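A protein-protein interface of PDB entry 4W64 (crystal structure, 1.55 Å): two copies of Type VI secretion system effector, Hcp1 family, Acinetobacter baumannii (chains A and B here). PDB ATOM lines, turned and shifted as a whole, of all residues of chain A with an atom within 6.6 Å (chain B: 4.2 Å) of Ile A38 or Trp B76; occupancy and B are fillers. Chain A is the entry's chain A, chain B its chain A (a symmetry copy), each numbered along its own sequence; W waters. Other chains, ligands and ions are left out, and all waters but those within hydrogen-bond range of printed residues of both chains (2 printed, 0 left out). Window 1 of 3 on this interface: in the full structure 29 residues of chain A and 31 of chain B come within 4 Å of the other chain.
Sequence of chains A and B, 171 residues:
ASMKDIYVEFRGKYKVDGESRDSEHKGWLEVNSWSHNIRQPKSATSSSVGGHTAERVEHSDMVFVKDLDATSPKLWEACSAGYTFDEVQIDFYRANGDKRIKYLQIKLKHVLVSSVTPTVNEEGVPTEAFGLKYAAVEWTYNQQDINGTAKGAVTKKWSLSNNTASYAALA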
ATOM      1  N   TRP A  34     -17.401  -7.467  10.622  1.00  0.00           N
ATOM      2  CA  TRP A  34     -16.064  -7.683  10.066  1.00  0.00           C
ATOM      3  C   TRP A  34     -15.284  -6.388  10.152  1.00  0.00           C
ATOM      4  O   TRP A  34     -15.833  -5.298   9.983  1.00  0.00           O
ATOM      5  CB  TRP A  34     -16.178  -8.106   8.604  1.00  0.00           C
ATOM      6  CG  TRP A  34     -14.903  -8.045   7.764  1.00  0.00           C
ATOM      7  CD1 TRP A  34     -13.876  -8.952   7.747  1.00  0.00           C
ATOM      8  CD2 TRP A  34     -14.591  -7.066   6.771  1.00  0.00           C
ATOM      9  NE1 TRP A  34     -12.924  -8.568   6.818  1.00  0.00           N
ATOM     10  CE2 TRP A  34     -13.345  -7.419   6.200  1.00  0.00           C
ATOM     11  CE3 TRP A  34     -15.238  -5.915   6.311  1.00  0.00           C
ATOM     12  CZ2 TRP A  34     -12.751  -6.667   5.187  1.00  0.00           C
ATOM     13  CZ3 TRP A  34     -14.647  -5.168   5.312  1.00  0.00           C
ATOM     14  CH2 TRP A  34     -13.410  -5.544   4.762  1.00  0.00           C
ATOM     15  N   HIS A  36     -11.060  -4.765   9.257  1.00  0.00           N
ATOM     16  CA  HIS A  36      -9.732  -5.017   8.710  1.00  0.00           C
ATOM     17  C   HIS A  36      -8.910  -3.744   8.758  1.00  0.00           C
ATOM     18  O   HIS A  36      -9.429  -2.670   9.106  1.00  0.00           O
ATOM     19  CB  HIS A  36      -9.823  -5.539   7.271  1.00  0.00           C
ATOM     20  CG  HIS A  36      -8.583  -6.223   6.798  1.00  0.00           C
ATOM     21  ND1 HIS A  36      -8.154  -6.166   5.482  1.00  0.00           N
ATOM     22  CD2 HIS A  36      -7.679  -6.987   7.452  1.00  0.00           C
ATOM     23  CE1 HIS A  36      -7.040  -6.858   5.360  1.00  0.00           C
ATOM     24  NE2 HIS A  36      -6.729  -7.373   6.542  1.00  0.00           N
ATOM     25  N   ASN A  37      -7.625  -3.868   8.428  1.00  0.00           N
ATOM     26  CA  ASN A  37      -6.715  -2.729   8.445  1.00  0.00           C
ATOM     27  C   ASN A  37      -5.544  -3.081   7.550  1.00  0.00           C
ATOM     28  O   ASN A  37      -5.024  -4.207   7.614  1.00  0.00           O
ATOM     29  CB  ASN A  37      -6.267  -2.452   9.887  1.00  0.00           C
ATOM     30  CG  ASN A  37      -5.483  -1.148  10.047  1.00  0.00           C
ATOM     31  OD1 ASN A  37      -4.650  -1.032  10.947  1.00  0.00           O
ATOM     32  ND2 ASN A  37      -5.760  -0.168   9.202  1.00  0.00           N
ATOM     33  N   ILE A  38      -5.152  -2.132   6.699  1.00  0.00           N
ATOM     34  CA  ILE A  38      -4.045  -2.306   5.771  1.00  0.00           C
ATOM     35  C   ILE A  38      -3.191  -1.059   5.895  1.00  0.00           C
ATOM     36  O   ILE A  38      -3.703   0.050   5.822  1.00  0.00           O
ATOM     37  CB  ILE A  38      -4.565  -2.424   4.328  1.00  0.00           C
ATOM     38  CG1 ILE A  38      -5.517  -3.619   4.198  1.00  0.00           C
ATOM     39  CG2 ILE A  38      -3.427  -2.548   3.348  1.00  0.00           C
ATOM     40  CD1 ILE A  38      -6.085  -3.799   2.780  1.00  0.00           C
ATOM     41  N   ARG A  39      -1.891  -1.232   6.099  1.00  0.00           N
ATOM     42  CA  ARG A  39      -1.005  -0.088   6.327  1.00  0.00           C
ATOM     43  C   ARG A  39       0.243  -0.195   5.464  1.00  0.00           C
ATOM     44  O   ARG A  39       0.964  -1.199   5.521  1.00  0.00           O
ATOM     45  CB  ARG A  39      -0.594  -0.011   7.794  1.00  0.00           C
ATOM     46  CG  ARG A  39      -1.749   0.184   8.767  1.00  0.00           C
ATOM     47  CD  ARG A  39      -1.209   0.418  10.164  1.00  0.00           C
ATOM     48  NE  ARG A  39      -2.267   0.522  11.161  1.00  0.00           N
ATOM     49  CZ  ARG A  39      -2.049   0.723  12.456  1.00  0.00           C
ATOM     50  NH1 ARG A  39      -0.807   0.839  12.907  1.00  0.00           N
ATOM     51  NH2 ARG A  39      -3.067   0.809  13.300  1.00  0.00           N
ATOM     52  N   GLN A  40       0.494   0.862   4.687  1.00  0.00           N
ATOM     53  CA  GLN A  40       1.602   0.936   3.734  1.00  0.00           C
ATOM     54  C   GLN A  40       2.631   1.951   4.220  1.00  0.00           C
ATOM     55  O   GLN A  40       2.348   3.145   4.272  1.00  0.00           O
ATOM     56  CB  GLN A  40       1.058   1.373   2.363  1.00  0.00           C
ATOM     57  CG  GLN A  40       2.124   1.625   1.286  1.00  0.00           C
ATOM     58  CD  GLN A  40       3.058   0.440   1.079  1.00  0.00           C
ATOM     59  OE1 GLN A  40       4.214   0.460   1.517  1.00  0.00           O
ATOM     60  NE2 GLN A  40       2.569  -0.595   0.402  1.00  0.00           N
ATOM     61  N   VAL A  57       3.748  -3.719   2.621  1.00  0.00           N
ATOM     62  CA  VAL A  57       2.497  -3.489   3.324  1.00  0.00           C
ATOM     63  C   VAL A  57       2.346  -4.436   4.515  1.00  0.00           C
ATOM     64  O   VAL A  57       2.888  -5.549   4.519  1.00  0.00           O
ATOM     65  CB  VAL A  57       1.299  -3.672   2.366  1.00  0.00           C
ATOM     66  CG1 VAL A  57       1.082  -5.149   2.039  1.00  0.00           C
ATOM     67  CG2 VAL A  57       0.045  -3.072   2.948  1.00  0.00           C
ATOM     68  N   GLU A  58       1.631  -3.973   5.534  1.00  0.00           N
ATOM     69  CA  GLU A  58       1.197  -4.828   6.627  1.00  0.00           C
ATOM     70  C   GLU A  58      -0.315  -4.984   6.542  1.00  0.00           C
ATOM     71  O   GLU A  58      -1.039  -3.987   6.624  1.00  0.00           O
ATOM     72  CB  GLU A  58       1.572  -4.210   7.978  1.00  0.00           C
ATOM     73  CG  GLU A  58       3.069  -4.106   8.224  1.00  0.00           C
ATOM     74  CD  GLU A  58       3.493  -2.747   8.765  1.00  0.00           C
ATOM     75  OE1 GLU A  58       2.809  -2.212   9.665  1.00  0.00           O
ATOM     76  OE2 GLU A  58       4.514  -2.210   8.282  1.00  0.00           O
ATOM     77  N   HIS A  59      -0.805  -6.212   6.349  1.00  0.00           N
ATOM     78  CA  HIS A  59      -2.230  -6.482   6.492  1.00  0.00           C
ATOM     79  C   HIS A  59      -2.484  -6.975   7.912  1.00  0.00           C
ATOM     80  O   HIS A  59      -1.819  -7.909   8.382  1.00  0.00           O
ATOM     81  CB  HIS A  59      -2.713  -7.586   5.533  1.00  0.00           C
ATOM     82  CG  HIS A  59      -2.924  -7.141   4.117  1.00  0.00           C
ATOM     83  ND1 HIS A  59      -3.793  -7.792   3.265  1.00  0.00           N
ATOM     84  CD2 HIS A  59      -2.359  -6.148   3.393  1.00  0.00           C
ATOM     85  CE1 HIS A  59      -3.760  -7.211   2.079  1.00  0.00           C
ATOM     86  NE2 HIS A  59      -2.894  -6.213   2.129  1.00  0.00           N
ATOM     87  N   SER A  60      -3.432  -6.353   8.602  1.00  0.00           N
ATOM     88  CA  SER A  60      -3.834  -6.853   9.910  1.00  0.00           C
ATOM     89  C   SER A  60      -4.685  -8.094   9.707  1.00  0.00           C
ATOM     90  O   SER A  60      -5.055  -8.424   8.569  1.00  0.00           O
ATOM     91  CB  SER A  60      -4.605  -5.779  10.674  1.00  0.00           C
ATOM     92  OG  SER A  60      -3.771  -4.658  10.930  1.00  0.00           O
ATOM     93  N   LEU A 104     -20.110  -7.799  -1.486  1.00  0.00           N
ATOM     94  CA  LEU A 104     -18.687  -8.012  -1.260  1.00  0.00           C
ATOM     95  C   LEU A 104     -18.425  -9.482  -1.068  1.00  0.00           C
ATOM     96  O   LEU A 104     -19.161 -10.158  -0.352  1.00  0.00           O
ATOM     97  CB  LEU A 104     -18.224  -7.230  -0.028  1.00  0.00           C
ATOM     98  CG  LEU A 104     -16.760  -7.360   0.420  1.00  0.00           C
ATOM     99  CD1 LEU A 104     -15.813  -6.892  -0.672  1.00  0.00           C
ATOM    100  CD2 LEU A 104     -16.533  -6.559   1.701  1.00  0.00           C
ATOM    101  N   ILE A 106     -14.970 -12.012  -0.247  1.00  0.00           N
ATOM    102  CA  ILE A 106     -13.536 -12.074   0.031  1.00  0.00           C
ATOM    103  C   ILE A 106     -13.093 -13.536   0.039  1.00  0.00           C
ATOM    104  O   ILE A 106     -13.731 -14.385   0.676  1.00  0.00           O
ATOM    105  CB  ILE A 106     -13.208 -11.430   1.393  1.00  0.00           C
ATOM    106  CG1 ILE A 106     -13.601  -9.955   1.355  1.00  0.00           C
ATOM    107  CG2 ILE A 106     -11.722 -11.599   1.734  1.00  0.00           C
ATOM    108  CD1 ILE A 106     -13.384  -9.200   2.678  1.00  0.00           C
ATOM    109  N   TYR A 134      -3.505 -14.776   6.675  1.00  0.00           N
ATOM    110  CA  TYR A 134      -3.535 -15.431   5.362  1.00  0.00           C
ATOM    111  C   TYR A 134      -2.343 -15.031   4.505  1.00  0.00           C
ATOM    112  O   TYR A 134      -1.677 -14.027   4.779  1.00  0.00           O
ATOM    113  CB  TYR A 134      -4.842 -15.053   4.629  1.00  0.00           C
ATOM    114  CG  TYR A 134      -5.054 -13.553   4.605  1.00  0.00           C
ATOM    115  CD1 TYR A 134      -4.537 -12.769   3.576  1.00  0.00           C
ATOM    116  CD2 TYR A 134      -5.723 -12.915   5.641  1.00  0.00           C
ATOM    117  CE1 TYR A 134      -4.702 -11.390   3.565  1.00  0.00           C
ATOM    118  CE2 TYR A 134      -5.873 -11.531   5.655  1.00  0.00           C
ATOM    119  CZ  TYR A 134      -5.363 -10.778   4.614  1.00  0.00           C
ATOM    120  OH  TYR A 134      -5.517  -9.404   4.619  1.00  0.00           O
ATOM    121  N   TRP A 139     -10.471  -9.833  -3.483  1.00  0.00           N
ATOM    122  CA  TRP A 139     -11.642  -9.063  -3.102  1.00  0.00           C
ATOM    123  C   TRP A 139     -12.507  -8.789  -4.327  1.00  0.00           C
ATOM    124  O   TRP A 139     -12.014  -8.285  -5.341  1.00  0.00           O
ATOM    125  CB  TRP A 139     -11.219  -7.700  -2.586  1.00  0.00           C
ATOM    126  CG  TRP A 139     -10.271  -7.604  -1.420  1.00  0.00           C
ATOM    127  CD1 TRP A 139     -10.578  -7.746  -0.084  1.00  0.00           C
ATOM    128  CD2 TRP A 139      -8.903  -7.186  -1.470  1.00  0.00           C
ATOM    129  NE1 TRP A 139      -9.469  -7.463   0.684  1.00  0.00           N
ATOM    130  CE2 TRP A 139      -8.427  -7.131  -0.146  1.00  0.00           C
ATOM    131  CE3 TRP A 139      -8.021  -6.880  -2.518  1.00  0.00           C
ATOM    132  CZ2 TRP A 139      -7.103  -6.777   0.165  1.00  0.00           C
ATOM    133  CZ3 TRP A 139      -6.706  -6.524  -2.202  1.00  0.00           C
ATOM    134  CH2 TRP A 139      -6.265  -6.474  -0.877  1.00  0.00           C
ATOM    135  N   THR A 140     -13.797  -9.082  -4.226  1.00  0.00           N
ATOM    136  CA  THR A 140     -14.721  -8.801  -5.319  1.00  0.00           C
ATOM    137  C   THR A 140     -15.872  -7.937  -4.824  1.00  0.00           C
ATOM    138  O   THR A 140     -16.577  -8.318  -3.881  1.00  0.00           O
ATOM    139  CB  THR A 140     -15.309 -10.094  -5.908  1.00  0.00           C
ATOM    140  OG1 THR A 140     -14.247 -10.952  -6.353  1.00  0.00           O
ATOM    141  CG2 THR A 140     -16.196  -9.767  -7.113  1.00  0.00           C
ATOM    142  N   TYR A 141     -16.072  -6.779  -5.450  1.00  0.00           N
ATOM    143  CA  TYR A 141     -17.186  -5.911  -5.085  1.00  0.00           C
ATOM    144  C   TYR A 141     -18.170  -5.878  -6.233  1.00  0.00           C
ATOM    145  O   TYR A 141     -17.807  -5.607  -7.384  1.00  0.00           O
ATOM    146  CB  TYR A 141     -16.722  -4.494  -4.729  1.00  0.00           C
ATOM    147  CG  TYR A 141     -17.802  -3.698  -4.026  1.00  0.00           C
ATOM    148  CD1 TYR A 141     -17.800  -3.562  -2.643  1.00  0.00           C
ATOM    149  CD2 TYR A 141     -18.826  -3.096  -4.749  1.00  0.00           C
ATOM    150  CE1 TYR A 141     -18.797  -2.849  -1.996  1.00  0.00           C
ATOM    151  CE2 TYR A 141     -19.820  -2.378  -4.112  1.00  0.00           C
ATOM    152  CZ  TYR A 141     -19.798  -2.264  -2.737  1.00  0.00           C
ATOM    153  OH  TYR A 141     -20.793  -1.554  -2.103  1.00  0.00           O
ATOM    154  N   LYS A 156     -10.029  -7.269  -7.266  1.00  0.00           N
ATOM    155  CA  LYS A 156      -8.645  -6.907  -7.001  1.00  0.00           C
ATOM    156  C   LYS A 156      -8.046  -7.964  -6.091  1.00  0.00           C
ATOM    157  O   LYS A 156      -8.770  -8.772  -5.511  1.00  0.00           O
ATOM    158  CB  LYS A 156      -8.579  -5.519  -6.345  1.00  0.00           C
ATOM    159  CG  LYS A 156      -9.113  -4.379  -7.201  1.00  0.00           C
ATOM    160  CD  LYS A 156      -8.263  -4.162  -8.443  1.00  0.00           C
ATOM    161  CE  LYS A 156      -8.773  -2.985  -9.252  1.00  0.00           C
ATOM    162  NZ  LYS A 156      -8.065  -2.891 -10.564  1.00  0.00           N
ATOM    163  N   TRP A 158      -4.260  -9.360  -3.674  1.00  0.00           N
ATOM    164  CA  TRP A 158      -2.909  -9.135  -3.178  1.00  0.00           C
ATOM    165  C   TRP A 158      -2.354 -10.410  -2.565  1.00  0.00           C
ATOM    166  O   TRP A 158      -3.054 -11.119  -1.830  1.00  0.00           O
ATOM    167  CB  TRP A 158      -2.855  -7.991  -2.153  1.00  0.00           C
ATOM    168  CG  TRP A 158      -1.430  -7.604  -1.906  1.00  0.00           C
ATOM    169  CD1 TRP A 158      -0.679  -7.850  -0.788  1.00  0.00           C
ATOM    170  CD2 TRP A 158      -0.565  -6.964  -2.840  1.00  0.00           C
ATOM    171  NE1 TRP A 158       0.602  -7.377  -0.972  1.00  0.00           N
ATOM    172  CE2 TRP A 158       0.695  -6.828  -2.225  1.00  0.00           C
ATOM    173  CE3 TRP A 158      -0.743  -6.472  -4.138  1.00  0.00           C
ATOM    174  CZ2 TRP A 158       1.772  -6.217  -2.869  1.00  0.00           C
ATOM    175  CZ3 TRP A 158       0.322  -5.880  -4.775  1.00  0.00           C
ATOM    176  CH2 TRP A 158       1.568  -5.754  -4.140  1.00  0.00           C
ATOM    177  N   SER B  72     -13.615   0.509  -3.086  1.00  0.00           N
ATOM    178  CA  SER B  72     -12.938  -0.073  -1.924  1.00  0.00           C
ATOM    179  C   SER B  72     -11.839  -1.091  -2.267  1.00  0.00           C
ATOM    180  O   SER B  72     -10.718  -0.943  -1.784  1.00  0.00           O
ATOM    181  CB  SER B  72     -13.941  -0.635  -0.900  1.00  0.00           C
ATOM    182  OG  SER B  72     -14.769   0.411  -0.404  1.00  0.00           O
ATOM    183  N   PRO B  73     -12.141  -2.106  -3.106  1.00  0.00           N
ATOM    184  CA  PRO B  73     -11.044  -3.034  -3.431  1.00  0.00           C
ATOM    185  C   PRO B  73      -9.923  -2.321  -4.178  1.00  0.00           C
ATOM    186  O   PRO B  73      -8.768  -2.750  -4.063  1.00  0.00           O
ATOM    187  CB  PRO B  73     -11.698  -4.062  -4.358  1.00  0.00           C
ATOM    188  CG  PRO B  73     -13.164  -3.957  -4.090  1.00  0.00           C
ATOM    189  CD  PRO B  73     -13.424  -2.537  -3.696  1.00  0.00           C
ATOM    190  N   LYS B  74     -10.248  -1.277  -4.937  1.00  0.00           N
ATOM    191  CA  LYS B  74      -9.222  -0.527  -5.656  1.00  0.00           C
ATOM    192  C   LYS B  74      -8.278   0.152  -4.664  1.00  0.00           C
ATOM    193  O   LYS B  74      -7.057   0.140  -4.858  1.00  0.00           O
ATOM    194  CB  LYS B  74      -9.855   0.511  -6.595  1.00  0.00           C
ATOM    195  CG  LYS B  74     -10.953  -0.062  -7.487  1.00  0.00           C
ATOM    196  CD  LYS B  74     -11.520   1.007  -8.433  1.00  0.00           C
ATOM    197  CE  LYS B  74     -12.664   0.438  -9.264  1.00  0.00           C
ATOM    198  NZ  LYS B  74     -13.164   1.437 -10.261  1.00  0.00           N
ATOM    199  N   LEU B  75      -8.841   0.729  -3.603  1.00  0.00           N
ATOM    200  CA  LEU B  75      -8.038   1.335  -2.549  1.00  0.00           C
ATOM    201  C   LEU B  75      -7.214   0.279  -1.811  1.00  0.00           C
ATOM    202  O   LEU B  75      -6.039   0.512  -1.488  1.00  0.00           O
ATOM    203  CB  LEU B  75      -8.925   2.097  -1.549  1.00  0.00           C
ATOM    204  CG  LEU B  75      -9.586   3.367  -2.088  1.00  0.00           C
ATOM    205  CD1 LEU B  75     -10.589   3.896  -1.077  1.00  0.00           C
ATOM    206  CD2 LEU B  75      -8.530   4.427  -2.372  1.00  0.00           C
ATOM    207  N   TRP B  76      -7.826  -0.870  -1.522  1.00  0.00           N
ATOM    208  CA  TRP B  76      -7.128  -1.929  -0.784  1.00  0.00           C
ATOM    209  C   TRP B  76      -5.918  -2.420  -1.561  1.00  0.00           C
ATOM    210  O   TRP B  76      -4.831  -2.616  -0.990  1.00  0.00           O
ATOM    211  CB  TRP B  76      -8.073  -3.099  -0.450  1.00  0.00           C
ATOM    212  CG  TRP B  76      -9.285  -2.651   0.340  1.00  0.00           C
ATOM    213  CD1 TRP B  76      -9.410  -1.505   1.063  1.00  0.00           C
ATOM    214  CD2 TRP B  76     -10.548  -3.333   0.445  1.00  0.00           C
ATOM    215  NE1 TRP B  76     -10.667  -1.435   1.630  1.00  0.00           N
ATOM    216  CE2 TRP B  76     -11.383  -2.547   1.263  1.00  0.00           C
ATOM    217  CE3 TRP B  76     -11.048  -4.536  -0.072  1.00  0.00           C
ATOM    218  CZ2 TRP B  76     -12.694  -2.918   1.576  1.00  0.00           C
ATOM    219  CZ3 TRP B  76     -12.354  -4.903   0.236  1.00  0.00           C
ATOM    220  CH2 TRP B  76     -13.161  -4.093   1.054  1.00  0.00           C
ATOM    221  N   GLU B  77      -6.089  -2.612  -2.867  1.00  0.00           N
ATOM    222  CA  GLU B  77      -4.961  -3.062  -3.682  1.00  0.00           C
ATOM    223  C   GLU B  77      -3.924  -1.949  -3.853  1.00  0.00           C
ATOM    224  O   GLU B  77      -2.725  -2.208  -3.763  1.00  0.00           O
ATOM    225  CB  GLU B  77      -5.426  -3.611  -5.039  1.00  0.00           C
ATOM    226  CG  GLU B  77      -4.292  -4.240  -5.859  1.00  0.00           C
ATOM    227  CD  GLU B  77      -4.732  -4.682  -7.240  1.00  0.00           C
ATOM    228  OE1 GLU B  77      -5.468  -5.687  -7.344  1.00  0.00           O
ATOM    229  OE2 GLU B  77      -4.330  -4.036  -8.231  1.00  0.00           O
ATOM    230  N   ALA B  78      -4.373  -0.719  -4.100  1.00  0.00           N
ATOM    231  CA  ALA B  78      -3.434   0.394  -4.279  1.00  0.00           C
ATOM    232  C   ALA B  78      -2.582   0.610  -3.032  1.00  0.00           C
ATOM    233  O   ALA B  78      -1.383   0.879  -3.124  1.00  0.00           O
ATOM    234  CB  ALA B  78      -4.177   1.672  -4.640  1.00  0.00           C
ATOM    235  N   CYS B  79      -3.203   0.515  -1.862  1.00  0.00           N
ATOM    236  CA  CYS B  79      -2.468   0.615  -0.613  1.00  0.00           C
ATOM    237  C   CYS B  79      -1.460  -0.522  -0.488  1.00  0.00           C
ATOM    238  O   CYS B  79      -0.296  -0.296  -0.152  1.00  0.00           O
ATOM    239  CB  CYS B  79      -3.452   0.577   0.560  1.00  0.00           C
ATOM    240  SG  CYS B  79      -2.698   0.852   2.171  1.00  0.00           S
ATOM    241  N   SER B  80      -1.902  -1.746  -0.773  1.00  0.00           N
ATOM    242  CA  SER B  80      -1.031  -2.917  -0.669  1.00  0.00           C
ATOM    243  C   SER B  80       0.188  -2.814  -1.583  1.00  0.00           C
ATOM    244  O   SER B  80       1.302  -3.141  -1.179  1.00  0.00           O
ATOM    245  CB  SER B  80      -1.823  -4.182  -1.002  1.00  0.00           C
ATOM    246  OG  SER B  80      -2.859  -4.382  -0.041  1.00  0.00           O
ATOM    247  N   SER B 115      -2.976   4.023   4.191  1.00  0.00           N
ATOM    248  CA  SER B 115      -3.738   3.121   5.047  1.00  0.00           C
ATOM    249  C   SER B 115      -5.164   3.031   4.560  1.00  0.00           C
ATOM    250  O   SER B 115      -5.684   3.967   3.959  1.00  0.00           O
ATOM    251  CB  SER B 115      -3.716   3.606   6.508  1.00  0.00           C
ATOM    252  OG  SER B 115      -4.412   4.842   6.654  1.00  0.00           O
ATOM    253  N   VAL B 116      -5.788   1.874   4.768  1.00  0.00           N
ATOM    254  CA  VAL B 116      -7.230   1.748   4.594  1.00  0.00           C
ATOM    255  C   VAL B 116      -7.768   0.862   5.700  1.00  0.00           C
ATOM    256  O   VAL B 116      -7.172  -0.178   6.044  1.00  0.00           O
ATOM    257  CB  VAL B 116      -7.645   1.140   3.240  1.00  0.00           C
ATOM    258  CG1 VAL B 116      -9.121   1.449   2.978  1.00  0.00           C
ATOM    259  CG2 VAL B 116      -6.774   1.649   2.102  1.00  0.00           C
ATOM    260  N   PRO B 118     -11.356  -0.693   6.678  1.00  0.00           N
ATOM    261  CA  PRO B 118     -12.781  -0.948   6.429  1.00  0.00           C
ATOM    262  C   PRO B 118     -13.472  -1.719   7.552  1.00  0.00           C
ATOM    263  O   PRO B 118     -12.862  -2.572   8.230  1.00  0.00           O
ATOM    264  CB  PRO B 118     -12.758  -1.779   5.135  1.00  0.00           C
ATOM    265  CG  PRO B 118     -11.473  -2.575   5.242  1.00  0.00           C
ATOM    266  CD  PRO B 118     -10.490  -1.666   5.966  1.00  0.00           C
ATOM    267  N   GLU B 128     -15.150   2.970   5.511  1.00  0.00           N
ATOM    268  CA  GLU B 128     -13.727   2.778   5.702  1.00  0.00           C
ATOM    269  C   GLU B 128     -13.057   4.127   5.849  1.00  0.00           C
ATOM    270  O   GLU B 128     -13.495   5.117   5.262  1.00  0.00           O
ATOM    271  CB  GLU B 128     -13.103   2.022   4.525  1.00  0.00           C
ATOM    272  CG  GLU B 128     -13.223   2.732   3.185  1.00  0.00           C
ATOM    273  CD  GLU B 128     -12.978   1.812   2.020  1.00  0.00           C
ATOM    274  OE1 GLU B 128     -13.348   2.191   0.886  1.00  0.00           O
ATOM    275  OE2 GLU B 128     -12.438   0.706   2.238  1.00  0.00           O
HETATM  276  O   HOH W   1       3.755  -4.134  -0.353  1.00  0.00           O
HETATM  277  O   HOH W   2      -5.548  -4.116 -10.791  1.00  0.00           O
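Printed residues of chain B within 4 Å of Ile A38: Trp B76, Cys B79, Ser B80, Ser B115 and Val B116. Of the printed residues of chain A, Trp B76 touches Trp A34 (3.99 Å), Ile A38 (3.9 Å) and Trp A139 (3.2 Å). Of the printed residues of chain B, Trp A34 touches Trp B76 (3.99 Å) and Pro B118 (3.6 Å). Printed residues of chain B within 4 Å of Asn A37: Val B116 (3.5 Å). Printed residues of chain B within 4 Å of Trp A139: Trp B76. Of the printed residues of chain B, Trp A158 touches Ser B80 (3.5 Å). Of the printed residues of chain A, Val B116 touches Asn A37 and Ile A38. The nearest printed residue of chain B that does not touch Ile A38 is Pro B118 (5.4 Å). The nearest printed residue of chain A that does not touch Cys B79 is Val A57 (4.2 Å).
The backbone NH (N) of His A36 is in hydrogen-bond range of the backbone carbonyl oxygen (O) of Pro B118, at 3.0 Å. The side-chain amide nitrogen (ND2) of Asn A37 sits at hydrogen-bond distance from the backbone carbonyl oxygen (O) of Val B116 (3.5 Å). The backbone carbonyl oxygen of Val B116 is in hydrogen-bond range of the backbone NH of Ile A38, at 2.9 Å. The side-chain amide nitrogen of Gln A40 lies within hydrogen-bond range of the backbone carbonyl oxygen of Cys B79. NE2 of Gln A40 is in hydrogen-bond range of O of Ser B80, at 3.3 Å. NE2 of His A59 is in hydrogen-bond range of OG of Ser B80 (2.8 Å).
No position is printed for both chains.
Among the printed residues, merely in contact across the chains: Ile A38 with Ser B115 (3.2 Å), Trp A139 with Trp B76 (3.2 Å), Lys A156 with Glu B77 (3.3 Å), Trp A158 with Ser B80 (3.5 Å), Lys A156 with Pro B73 (3.6 Å), Trp A34 with Pro B118 (3.6 Å), Val A57 with Ser B80 (3.6 Å), Tyr A141 with Pro B73 (3.7 Å), Ile A38 with Cys B79 (3.7 Å), Ile A38 with Trp B76 (3.9 Å), Ile A38 with Ser B80 (3.9 Å) and Trp A34 with Trp B76 (3.99 Å).
Of the 18 printed residues of chain A, 11 touch a printed residue of chain B. Hydrophobic or aromatic side chains of chain A that line the printed part of chain B: Trp A34, His A36, Ile A38, Val A57, His A59, Trp A139, Tyr A141 and Trp A158. Printed residues of chain B that touch a printed residue of chain A: Pro B73, Trp B76, Glu B77, Cys B79, Ser B80, Ser B115, Val B116 and Pro B118. Hydrophobic or aromatic side chains of chain B that line the printed part of chain A: Pro B73, Trp B76 and Pro B118. Among the printed residues, no Asp or Glu carboxylate lies within 4 Å of a Lys or Arg side-chain nitrogen of the other chain.
OD1 of Asn A37 sits at hydrogen-bond distance from NE of Arg A39 (2.9 Å). N of Ser A60 lies within hydrogen-bond range of O of Asn A37 (2.8 Å). O of Lys A156 sits at hydrogen-bond distance from N of Trp A139 (2.9 Å). O of Ser B72 lies close to NE1 of Trp B76, 3.4 Å away. O of Trp B76 lies within hydrogen-bond range of OG of Ser B80, at 2.8 Å. NE1 of Trp B76 is in hydrogen-bond range of OE2 of Glu B128, 2.8 Å away.
Water W1 lies within hydrogen-bond range of O of Ser B80 (2.8 Å) and N of Val A57 (3.0 Å). Water W2 lies within hydrogen-bond range of NZ of Lys A156 (2.8 Å) and OE2 of Glu B77 (2.8 Å).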
